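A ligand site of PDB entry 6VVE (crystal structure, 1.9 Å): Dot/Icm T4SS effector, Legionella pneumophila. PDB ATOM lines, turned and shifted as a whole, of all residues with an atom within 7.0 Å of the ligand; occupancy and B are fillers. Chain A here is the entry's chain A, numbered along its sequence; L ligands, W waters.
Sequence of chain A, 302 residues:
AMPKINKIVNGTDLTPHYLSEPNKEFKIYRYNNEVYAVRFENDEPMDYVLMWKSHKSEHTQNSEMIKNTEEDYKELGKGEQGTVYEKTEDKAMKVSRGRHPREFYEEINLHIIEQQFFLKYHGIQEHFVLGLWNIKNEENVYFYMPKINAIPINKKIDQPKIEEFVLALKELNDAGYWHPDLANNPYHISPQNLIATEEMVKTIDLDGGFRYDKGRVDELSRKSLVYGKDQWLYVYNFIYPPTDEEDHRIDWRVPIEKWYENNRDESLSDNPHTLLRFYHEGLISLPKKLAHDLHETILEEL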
ATOM      1  N   THR A  12     -33.457   2.447   6.285  1.00  0.00           N
ATOM      2  CA  THR A  12     -33.083   1.030   6.331  1.00  0.00           C
ATOM      3  C   THR A  12     -31.594   0.923   6.613  1.00  0.00           C
ATOM      4  O   THR A  12     -30.762   1.480   5.874  1.00  0.00           O
ATOM      5  CB  THR A  12     -33.438   0.328   5.018  1.00  0.00           C
ATOM      6  OG1 THR A  12     -34.802   0.586   4.688  1.00  0.00           O
ATOM      7  CG2 THR A  12     -33.222  -1.170   5.142  1.00  0.00           C
ATOM      8  N   ASP A  13     -31.236   0.180   7.663  1.00  0.00           N
ATOM      9  CA  ASP A  13     -29.845   0.031   8.079  1.00  0.00           C
ATOM     10  C   ASP A  13     -29.173  -1.002   7.180  1.00  0.00           C
ATOM     11  O   ASP A  13     -29.488  -2.192   7.253  1.00  0.00           O
ATOM     12  CB  ASP A  13     -29.791  -0.378   9.548  1.00  0.00           C
ATOM     13  CG  ASP A  13     -28.383  -0.377  10.099  1.00  0.00           C
ATOM     14  OD1 ASP A  13     -27.419  -0.414   9.307  1.00  0.00           O
ATOM     15  OD2 ASP A  13     -28.237  -0.353  11.345  1.00  0.00           O
ATOM     16  N   LEU A  14     -28.232  -0.550   6.357  1.00  0.00           N
ATOM     17  CA  LEU A  14     -27.454  -1.417   5.476  1.00  0.00           C
ATOM     18  C   LEU A  14     -26.049  -1.690   6.011  1.00  0.00           C
ATOM     19  O   LEU A  14     -25.236  -2.311   5.308  1.00  0.00           O
ATOM     20  CB  LEU A  14     -27.360  -0.801   4.075  1.00  0.00           C
ATOM     21  CG  LEU A  14     -28.636  -0.263   3.448  1.00  0.00           C
ATOM     22  CD1 LEU A  14     -28.330   0.315   2.064  1.00  0.00           C
ATOM     23  CD2 LEU A  14     -29.715  -1.331   3.348  1.00  0.00           C
ATOM     24  N   HIS A  17     -23.849  -4.857   5.468  1.00  0.00           N
ATOM     25  CA  HIS A  17     -23.419  -5.135   4.109  1.00  0.00           C
ATOM     26  C   HIS A  17     -22.179  -4.352   3.689  1.00  0.00           C
ATOM     27  O   HIS A  17     -21.753  -4.474   2.533  1.00  0.00           O
ATOM     28  CB  HIS A  17     -24.556  -4.823   3.121  1.00  0.00           C
ATOM     29  CG  HIS A  17     -25.763  -5.671   3.309  1.00  0.00           C
ATOM     30  ND1 HIS A  17     -26.964  -5.405   2.688  1.00  0.00           N
ATOM     31  CD2 HIS A  17     -25.970  -6.788   4.047  1.00  0.00           C
ATOM     32  CE1 HIS A  17     -27.849  -6.320   3.033  1.00  0.00           C
ATOM     33  NE2 HIS A  17     -27.277  -7.171   3.861  1.00  0.00           N
ATOM     34  N   TYR A  18     -21.595  -3.555   4.594  1.00  0.00           N
ATOM     35  CA  TYR A  18     -20.494  -2.673   4.219  1.00  0.00           C
ATOM     36  C   TYR A  18     -19.435  -2.540   5.300  1.00  0.00           C
ATOM     37  O   TYR A  18     -18.239  -2.437   5.001  1.00  0.00           O
ATOM     38  CB  TYR A  18     -21.055  -1.284   3.847  1.00  0.00           C
ATOM     39  CG  TYR A  18     -21.875  -1.283   2.578  1.00  0.00           C
ATOM     40  CD1 TYR A  18     -21.266  -1.407   1.339  1.00  0.00           C
ATOM     41  CD2 TYR A  18     -23.255  -1.162   2.629  1.00  0.00           C
ATOM     42  CE1 TYR A  18     -22.021  -1.409   0.165  1.00  0.00           C
ATOM     43  CE2 TYR A  18     -24.012  -1.160   1.465  1.00  0.00           C
ATOM     44  CZ  TYR A  18     -23.387  -1.283   0.240  1.00  0.00           C
ATOM     45  OH  TYR A  18     -24.139  -1.301  -0.915  1.00  0.00           O
ATOM     46  N   ILE A  28     -24.638   2.879   7.770  1.00  0.00           N
ATOM     47  CA  ILE A  28     -25.100   3.081   6.395  1.00  0.00           C
ATOM     48  C   ILE A  28     -26.615   2.930   6.384  1.00  0.00           C
ATOM     49  O   ILE A  28     -27.152   1.912   6.862  1.00  0.00           O
ATOM     50  CB  ILE A  28     -24.442   2.090   5.420  1.00  0.00           C
ATOM     51  CG1 ILE A  28     -22.922   2.152   5.523  1.00  0.00           C
ATOM     52  CG2 ILE A  28     -24.913   2.376   4.000  1.00  0.00           C
ATOM     53  CD1 ILE A  28     -22.327   3.490   5.168  1.00  0.00           C
ATOM     54  N   ARG A  30     -30.288   3.570   3.942  1.00  0.00           N
ATOM     55  CA  ARG A  30     -31.030   3.923   2.744  1.00  0.00           C
ATOM     56  C   ARG A  30     -32.266   4.710   3.169  1.00  0.00           C
ATOM     57  O   ARG A  30     -33.115   4.190   3.911  1.00  0.00           O
ATOM     58  CB  ARG A  30     -31.429   2.681   1.941  1.00  0.00           C
ATOM     59  CG  ARG A  30     -31.979   3.017   0.557  1.00  0.00           C
ATOM     60  CD  ARG A  30     -32.346   1.757  -0.253  1.00  0.00           C
ATOM     61  NE  ARG A  30     -32.905   0.707   0.597  1.00  0.00           N
ATOM     62  CZ  ARG A  30     -32.360  -0.498   0.771  1.00  0.00           C
ATOM     63  NH1 ARG A  30     -31.237  -0.833   0.149  1.00  0.00           N
ATOM     64  NH2 ARG A  30     -32.948  -1.377   1.568  1.00  0.00           N
ATOM     65  N   GLU A  34     -31.879   7.069  -1.370  1.00  0.00           N
ATOM     66  CA  GLU A  34     -30.547   7.620  -1.243  1.00  0.00           C
ATOM     67  C   GLU A  34     -29.820   6.864  -0.134  1.00  0.00           C
ATOM     68  O   GLU A  34     -30.361   6.686   0.953  1.00  0.00           O
ATOM     69  CB  GLU A  34     -30.587   9.117  -0.911  1.00  0.00           C
ATOM     70  CG  GLU A  34     -31.331   9.971  -1.930  1.00  0.00           C
ATOM     71  CD  GLU A  34     -30.629  10.004  -3.284  1.00  0.00           C
ATOM     72  OE1 GLU A  34     -29.462   9.562  -3.365  1.00  0.00           O
ATOM     73  OE2 GLU A  34     -31.269  10.463  -4.264  1.00  0.00           O
ATOM     74  N   VAL A  35     -28.599   6.427  -0.425  1.00  0.00           N
ATOM     75  CA  VAL A  35     -27.772   5.709   0.541  1.00  0.00           C
ATOM     76  C   VAL A  35     -26.803   6.689   1.177  1.00  0.00           C
ATOM     77  O   VAL A  35     -25.995   7.316   0.471  1.00  0.00           O
ATOM     78  CB  VAL A  35     -27.026   4.542  -0.132  1.00  0.00           C
ATOM     79  CG1 VAL A  35     -26.005   3.943   0.827  1.00  0.00           C
ATOM     80  CG2 VAL A  35     -28.018   3.477  -0.586  1.00  0.00           C
ATOM     81  N   TRP A  52     -24.781   7.399  -2.846  1.00  0.00           N
ATOM     82  CA  TRP A  52     -25.318   7.200  -4.183  1.00  0.00           C
ATOM     83  C   TRP A  52     -26.844   7.115  -4.101  1.00  0.00           C
ATOM     84  O   TRP A  52     -27.427   7.044  -3.011  1.00  0.00           O
ATOM     85  CB  TRP A  52     -24.744   5.935  -4.840  1.00  0.00           C
ATOM     86  CG  TRP A  52     -25.031   4.663  -4.097  1.00  0.00           C
ATOM     87  CD1 TRP A  52     -26.202   3.954  -4.086  1.00  0.00           C
ATOM     88  CD2 TRP A  52     -24.110   3.934  -3.269  1.00  0.00           C
ATOM     89  NE1 TRP A  52     -26.077   2.839  -3.295  1.00  0.00           N
ATOM     90  CE2 TRP A  52     -24.800   2.802  -2.776  1.00  0.00           C
ATOM     91  CE3 TRP A  52     -22.779   4.132  -2.882  1.00  0.00           C
ATOM     92  CZ2 TRP A  52     -24.201   1.879  -1.923  1.00  0.00           C
ATOM     93  CZ3 TRP A  52     -22.185   3.215  -2.044  1.00  0.00           C
ATOM     94  CH2 TRP A  52     -22.899   2.092  -1.572  1.00  0.00           C
ATOM     95  N   LYS A  53     -27.482   7.132  -5.273  1.00  0.00           N
ATOM     96  CA  LYS A  53     -28.922   7.006  -5.384  1.00  0.00           C
ATOM     97  C   LYS A  53     -29.295   5.540  -5.594  1.00  0.00           C
ATOM     98  O   LYS A  53     -28.615   4.812  -6.313  1.00  0.00           O
ATOM     99  CB  LYS A  53     -29.455   7.856  -6.545  1.00  0.00           C
ATOM    100  CG  LYS A  53     -30.970   7.868  -6.675  1.00  0.00           C
ATOM    101  CD  LYS A  53     -31.444   8.955  -7.636  1.00  0.00           C
ATOM    102  CE  LYS A  53     -32.967   9.004  -7.760  1.00  0.00           C
ATOM    103  NZ  LYS A  53     -33.612   9.742  -6.639  1.00  0.00           N
ATOM    104  N   SER A  54     -30.378   5.123  -4.944  1.00  0.00           N
ATOM    105  CA  SER A  54     -30.801   3.732  -4.931  1.00  0.00           C
ATOM    106  C   SER A  54     -32.131   3.558  -5.659  1.00  0.00           C
ATOM    107  O   SER A  54     -33.006   4.430  -5.591  1.00  0.00           O
ATOM    108  CB  SER A  54     -30.939   3.225  -3.486  1.00  0.00           C
ATOM    109  OG  SER A  54     -31.697   2.020  -3.414  1.00  0.00           O
ATOM    110  N   HIS A  55     -32.285   2.416  -6.336  1.00  0.00           N
ATOM    111  CA  HIS A  55     -33.525   2.037  -6.981  1.00  0.00           C
ATOM    112  C   HIS A  55     -34.145   0.801  -6.341  1.00  0.00           C
ATOM    113  O   HIS A  55     -34.958   0.112  -6.972  1.00  0.00           O
ATOM    114  CB  HIS A  55     -33.301   1.799  -8.477  1.00  0.00           C
ATOM    115  CG  HIS A  55     -33.009   3.037  -9.250  1.00  0.00           C
ATOM    116  ND1 HIS A  55     -33.785   3.465 -10.310  1.00  0.00           N
ATOM    117  CD2 HIS A  55     -32.015   3.958  -9.126  1.00  0.00           C
ATOM    118  CE1 HIS A  55     -33.288   4.586 -10.794  1.00  0.00           C
ATOM    119  NE2 HIS A  55     -32.218   4.911 -10.095  1.00  0.00           N
ATOM    120  N   LYS A  56     -33.779   0.498  -5.096  1.00  0.00           N
ATOM    121  CA  LYS A  56     -34.317  -0.657  -4.388  1.00  0.00           C
ATOM    122  C   LYS A  56     -35.837  -0.719  -4.457  1.00  0.00           C
ATOM    123  O   LYS A  56     -36.506   0.302  -4.360  1.00  0.00           O
ATOM    124  CB  LYS A  56     -33.848  -0.628  -2.925  1.00  0.00           C
ATOM    125  CG  LYS A  56     -34.704  -1.408  -1.939  1.00  0.00           C
ATOM    126  CD  LYS A  56     -34.819  -2.873  -2.303  1.00  0.00           C
ATOM    127  CE  LYS A  56     -35.339  -3.690  -1.125  1.00  0.00           C
ATOM    128  NZ  LYS A  56     -34.441  -4.837  -0.813  1.00  0.00           N
ATOM    129  N   TYR A  73     -25.282  -7.600 -17.037  1.00  0.00           N
ATOM    130  CA  TYR A  73     -25.303  -6.158 -16.855  1.00  0.00           C
ATOM    131  C   TYR A  73     -24.535  -5.488 -17.999  1.00  0.00           C
ATOM    132  O   TYR A  73     -23.592  -6.044 -18.559  1.00  0.00           O
ATOM    133  CB  TYR A  73     -24.683  -5.762 -15.519  1.00  0.00           C
ATOM    134  CG  TYR A  73     -25.511  -6.142 -14.317  1.00  0.00           C
ATOM    135  CD1 TYR A  73     -26.696  -5.476 -14.030  1.00  0.00           C
ATOM    136  CD2 TYR A  73     -25.102  -7.140 -13.453  1.00  0.00           C
ATOM    137  CE1 TYR A  73     -27.459  -5.817 -12.926  1.00  0.00           C
ATOM    138  CE2 TYR A  73     -25.855  -7.495 -12.352  1.00  0.00           C
ATOM    139  CZ  TYR A  73     -27.029  -6.821 -12.097  1.00  0.00           C
ATOM    140  OH  TYR A  73     -27.780  -7.167 -11.000  1.00  0.00           O
ATOM    141  N   LYS A  87     -25.252  -0.848 -12.839  1.00  0.00           N
ATOM    142  CA  LYS A  87     -26.295  -1.473 -12.018  1.00  0.00           C
ATOM    143  C   LYS A  87     -27.633  -0.791 -12.253  1.00  0.00           C
ATOM    144  O   LYS A  87     -28.648  -1.456 -12.461  1.00  0.00           O
ATOM    145  CB  LYS A  87     -25.890  -1.414 -10.540  1.00  0.00           C
ATOM    146  CG  LYS A  87     -26.859  -2.101  -9.599  1.00  0.00           C
ATOM    147  CD  LYS A  87     -26.997  -3.581  -9.929  1.00  0.00           C
ATOM    148  CE  LYS A  87     -27.585  -4.367  -8.759  1.00  0.00           C
ATOM    149  NZ  LYS A  87     -29.053  -4.194  -8.641  1.00  0.00           N
ATOM    150  N   THR A  88     -27.648   0.545 -12.194  1.00  0.00           N
ATOM    151  CA  THR A  88     -28.832   1.337 -12.520  1.00  0.00           C
ATOM    152  C   THR A  88     -28.378   2.557 -13.310  1.00  0.00           C
ATOM    153  O   THR A  88     -27.182   2.769 -13.540  1.00  0.00           O
ATOM    154  CB  THR A  88     -29.605   1.749 -11.261  1.00  0.00           C
ATOM    155  OG1 THR A  88     -28.834   2.692 -10.507  1.00  0.00           O
ATOM    156  CG2 THR A  88     -29.914   0.536 -10.392  1.00  0.00           C
ATOM    157  N   LYS A  91     -26.122   4.391 -10.752  1.00  0.00           N
ATOM    158  CA  LYS A  91     -25.144   3.703  -9.924  1.00  0.00           C
ATOM    159  C   LYS A  91     -24.293   2.762 -10.757  1.00  0.00           C
ATOM    160  O   LYS A  91     -24.833   1.956 -11.536  1.00  0.00           O
ATOM    161  CB  LYS A  91     -25.852   2.914  -8.808  1.00  0.00           C
ATOM    162  CG  LYS A  91     -24.914   2.200  -7.858  1.00  0.00           C
ATOM    163  CD  LYS A  91     -25.660   1.598  -6.692  1.00  0.00           C
ATOM    164  CE  LYS A  91     -26.550   0.451  -7.131  1.00  0.00           C
ATOM    165  NZ  LYS A  91     -27.196  -0.229  -5.974  1.00  0.00           N
ATOM    166  N   MET A  93     -21.033  -0.180 -10.808  1.00  0.00           N
ATOM    167  CA  MET A  93     -20.667  -1.362 -10.037  1.00  0.00           C
ATOM    168  C   MET A  93     -19.386  -1.987 -10.592  1.00  0.00           C
ATOM    169  O   MET A  93     -19.355  -2.480 -11.718  1.00  0.00           O
ATOM    170  CB  MET A  93     -21.819  -2.377 -10.089  1.00  0.00           C
ATOM    171  CG  MET A  93     -21.633  -3.634  -9.237  1.00  0.00           C
ATOM    172  SD  MET A  93     -23.196  -4.724  -9.380  1.00  0.00           S
ATOM    173  CE  MET A  93     -23.029  -6.014  -8.000  1.00  0.00           C
ATOM    174  N   ASN A 134     -19.386  -3.622  -1.300  1.00  0.00           N
ATOM    175  CA  ASN A 134     -20.429  -4.483  -0.763  1.00  0.00           C
ATOM    176  C   ASN A 134     -19.830  -5.842  -0.437  1.00  0.00           C
ATOM    177  O   ASN A 134     -19.222  -6.487  -1.306  1.00  0.00           O
ATOM    178  CB  ASN A 134     -21.566  -4.616  -1.765  1.00  0.00           C
ATOM    179  CG  ASN A 134     -22.808  -5.248  -1.150  1.00  0.00           C
ATOM    180  OD1 ASN A 134     -22.799  -6.432  -0.794  1.00  0.00           O
ATOM    181  ND2 ASN A 134     -23.877  -4.470  -1.031  1.00  0.00           N
ATOM    182  N   LYS A 136     -21.552  -8.352   1.650  1.00  0.00           N
ATOM    183  CA  LYS A 136     -22.496  -9.286   2.252  1.00  0.00           C
ATOM    184  C   LYS A 136     -22.237 -10.716   1.775  1.00  0.00           C
ATOM    185  O   LYS A 136     -22.573 -11.680   2.473  1.00  0.00           O
ATOM    186  CB  LYS A 136     -23.940  -8.857   1.966  1.00  0.00           C
ATOM    187  CG  LYS A 136     -24.359  -8.908   0.503  1.00  0.00           C
ATOM    188  CD  LYS A 136     -25.637  -8.091   0.320  1.00  0.00           C
ATOM    189  CE  LYS A 136     -26.149  -8.157  -1.118  1.00  0.00           C
ATOM    190  NZ  LYS A 136     -27.384  -7.351  -1.308  1.00  0.00           N
ATOM    191  N   TYR A 142     -18.093  -6.261  -4.569  1.00  0.00           N
ATOM    192  CA  TYR A 142     -18.177  -5.294  -5.645  1.00  0.00           C
ATOM    193  C   TYR A 142     -18.318  -3.904  -5.055  1.00  0.00           C
ATOM    194  O   TYR A 142     -18.729  -3.742  -3.899  1.00  0.00           O
ATOM    195  CB  TYR A 142     -19.351  -5.591  -6.581  1.00  0.00           C
ATOM    196  CG  TYR A 142     -20.643  -5.911  -5.870  1.00  0.00           C
ATOM    197  CD1 TYR A 142     -21.480  -4.902  -5.403  1.00  0.00           C
ATOM    198  CD2 TYR A 142     -21.034  -7.234  -5.665  1.00  0.00           C
ATOM    199  CE1 TYR A 142     -22.656  -5.191  -4.750  1.00  0.00           C
ATOM    200  CE2 TYR A 142     -22.221  -7.531  -5.012  1.00  0.00           C
ATOM    201  CZ  TYR A 142     -23.020  -6.514  -4.560  1.00  0.00           C
ATOM    202  OH  TYR A 142     -24.204  -6.805  -3.919  1.00  0.00           O
ATOM    203  N   TYR A 144     -19.908  -0.248  -5.205  1.00  0.00           N
ATOM    204  CA  TYR A 144     -20.979   0.639  -5.660  1.00  0.00           C
ATOM    205  C   TYR A 144     -20.485   2.077  -5.683  1.00  0.00           C
ATOM    206  O   TYR A 144     -19.721   2.504  -4.807  1.00  0.00           O
ATOM    207  CB  TYR A 144     -22.202   0.530  -4.758  1.00  0.00           C
ATOM    208  CG  TYR A 144     -23.166  -0.594  -5.049  1.00  0.00           C
ATOM    209  CD1 TYR A 144     -23.311  -1.114  -6.333  1.00  0.00           C
ATOM    210  CD2 TYR A 144     -23.943  -1.135  -4.037  1.00  0.00           C
ATOM    211  CE1 TYR A 144     -24.191  -2.148  -6.593  1.00  0.00           C
ATOM    212  CE2 TYR A 144     -24.836  -2.173  -4.287  1.00  0.00           C
ATOM    213  CZ  TYR A 144     -24.956  -2.668  -5.575  1.00  0.00           C
ATOM    214  OH  TYR A 144     -25.839  -3.685  -5.819  1.00  0.00           O
HETATM  215  C1  LIG L   1     -30.265  -2.591  -4.790  1.00  0.00           C
HETATM  216  C2  LIG L   1     -31.242  -3.774  -4.784  1.00  0.00           C
HETATM  217  C3  LIG L   1     -30.683  -4.958  -3.995  1.00  0.00           C
HETATM  218  C4  LIG L   1     -30.343  -4.546  -2.562  1.00  0.00           C
HETATM  219  C5  LIG L   1     -29.265  -3.431  -2.580  1.00  0.00           C
HETATM  220  C6  LIG L   1     -29.717  -2.228  -3.404  1.00  0.00           C
HETATM  221  O1  LIG L   1     -30.928  -1.450  -5.291  1.00  0.00           O
HETATM  222  P1  LIG L   1     -30.540  -0.905  -6.785  1.00  0.00           P
HETATM  223  O2  LIG L   1     -30.406   0.599  -6.741  1.00  0.00           O
HETATM  224  O3  LIG L   1     -29.247  -1.530  -7.237  1.00  0.00           O
HETATM  225  O4  LIG L   1     -31.647  -1.283  -7.760  1.00  0.00           O
HETATM  226  O5  LIG L   1     -31.450  -4.161  -6.126  1.00  0.00           O
HETATM  227  P2  LIG L   1     -32.996  -4.296  -6.683  1.00  0.00           P
HETATM  228  O6  LIG L   1     -33.961  -3.770  -5.651  1.00  0.00           O
HETATM  229  O7  LIG L   1     -33.134  -3.500  -7.949  1.00  0.00           O
HETATM  230  O8  LIG L   1     -33.299  -5.752  -6.945  1.00  0.00           O
HETATM  231  O9  LIG L   1     -29.516  -5.390  -4.622  1.00  0.00           O
HETATM  232  P3  LIG L   1     -29.242  -6.990  -4.863  1.00  0.00           P
HETATM  233  O10 LIG L   1     -30.508  -7.779  -4.602  1.00  0.00           O
HETATM  234  O11 LIG L   1     -28.791  -7.192  -6.302  1.00  0.00           O
HETATM  235  O12 LIG L   1     -28.146  -7.477  -3.939  1.00  0.00           O
HETATM  236  O13 LIG L   1     -29.857  -5.643  -1.848  1.00  0.00           O
HETATM  237  P4  LIG L   1     -30.518  -5.933  -0.372  1.00  0.00           P
HETATM  238  O14 LIG L   1     -31.997  -6.211  -0.511  1.00  0.00           O
HETATM  239  O15 LIG L   1     -30.349  -4.698   0.495  1.00  0.00           O
HETATM  240  O16 LIG L   1     -29.838  -7.119   0.263  1.00  0.00           O
HETATM  241  O17 LIG L   1     -29.009  -3.015  -1.281  1.00  0.00           O
HETATM  242  P5  LIG L   1     -27.559  -3.358  -0.607  1.00  0.00           P
HETATM  243  O18 LIG L   1     -27.735  -3.583   0.884  1.00  0.00           O
HETATM  244  O19 LIG L   1     -26.963  -4.593  -1.226  1.00  0.00           O
HETATM  245  O20 LIG L   1     -26.628  -2.179  -0.844  1.00  0.00           O
HETATM  246  O21 LIG L   1     -28.615  -1.366  -3.582  1.00  0.00           O
HETATM  247  P6  LIG L   1     -28.599   0.101  -2.825  1.00  0.00           P
HETATM  248  O22 LIG L   1     -28.263   1.189  -3.826  1.00  0.00           O
HETATM  249  O23 LIG L   1     -29.938   0.374  -2.203  1.00  0.00           O
HETATM  250  O24 LIG L   1     -27.539   0.053  -1.739  1.00  0.00           O
HETATM  251  O   HOH W   1     -29.136   2.867  -7.780  1.00  0.00           O
HETATM  252  O   HOH W   2     -32.985  -3.770   2.518  1.00  0.00           O
HETATM  253  O   HOH W   3     -26.232  -5.421  -3.551  1.00  0.00           O
HETATM  254  O   HOH W   4     -34.415  -5.489  -3.693  1.00  0.00           O
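Residues that only touch the ligand: Thr 88, Val 35, Leu 14, Tyr 144 and Tyr 142.
Hydrophobic or aromatic side chains within 4 Å of the ligand: Leu 14, His 17, Tyr 18, Val 35, Trp 52, His 55 and Tyr 144.
Within 4 Å of the ligand: Leu 14, His 17, Tyr 18, Arg 30, Val 35, Trp 52, Ser 54, His 55, Lys 56, Lys 87, Thr 88, Lys 91, Asn 134, Lys 136, Tyr 142 and Tyr 144.
The side-chain hydroxyl (OH) of Tyr 18 is in hydrogen-bond range of an oxygen (O20) of the ligand (2.6 Å).
An oxygen (O2) of the ligand is in hydrogen-bond range of the backbone NH (N) of His 55 (2.6 Å).
A ring nitrogen (ND1) of His 17 is in hydrogen-bond range of an oxygen (O18) of the ligand (2.7 Å).
An oxygen (O23) of the ligand sits at hydrogen-bond distance from the side-chain hydroxyl (OG) of Ser 54 (2.7 Å).
An oxygen (O3) of the ligand lies within salt-bridge range of the side-chain amino group (NZ) of Lys 91 (2.7 Å).
An oxygen (O12) of the ligand lies within salt-bridge range of the side-chain amino group of Lys 136, 2.7 Å away.
NE1 of Trp 52 is in hydrogen-bond range of O22 of the ligand (2.8 Å).
The backbone NH (N) of Lys 56 lies within hydrogen-bond range of an oxygen (O1) of the ligand.
The side-chain amino group of Lys 56 is in salt-bridge range of an oxygen (O14) of the ligand.
NH1 of Arg 30 lies within salt-bridge range of O23 of the ligand.
NZ of Lys 87 is in salt-bridge range of O3 of the ligand.
The side-chain amide nitrogen (ND2) of Asn 134 lies within hydrogen-bond range of an oxygen (O19) of the ligand.
Water W3 lies within hydrogen-bond range of the side-chain hydroxyl of Tyr 142 (2.5 Å), an oxygen (O19) of the ligand (2.6 Å), the side-chain hydroxyl of Tyr 144 (2.9 Å) and the side-chain amino group of Lys 136 (3.2 Å).
Water W4 bridges an oxygen (O6) of the ligand (2.6 Å) and the side-chain amino group (NZ) of Lys 56 (3.0 Å).
Water W1 lies within hydrogen-bond range of the backbone carbonyl oxygen of Lys 53 (2.5 Å), the side-chain hydroxyl of Thr 88 (2.7 Å), an oxygen (O2) of the ligand (2.8 Å) and the backbone NH of His 55 (3.5 Å).
Water W2 bridges NH2 of Arg 30 (2.6 Å) and O15 of the ligand (3.4 Å).
The side-chain hydroxyl of Tyr 18 is in hydrogen-bond range of the side-chain amide nitrogen of Asn 134 (3.2 Å).
N of Lys 56 lies within hydrogen-bond range of OG of Ser 54 (3.1 Å).
The backbone NH of Lys 91 sits at hydrogen-bond distance from the side-chain hydroxyl of Thr 88, at 3.2 Å.
OD1 of Asn 134 lies close to N of Lys 136 (3.3 Å).
O of Trp 52 is in hydrogen-bond range of N of Val 35, at 2.9 Å.
The backbone NH of Arg 30 is in hydrogen-bond range of the backbone carbonyl oxygen of Thr 12 (2.9 Å).
O of Tyr 142 lies within hydrogen-bond range of N of Asn 134 (2.7 Å).
N of Leu 14 sits at hydrogen-bond distance from O of Ile 28 (2.7 Å).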
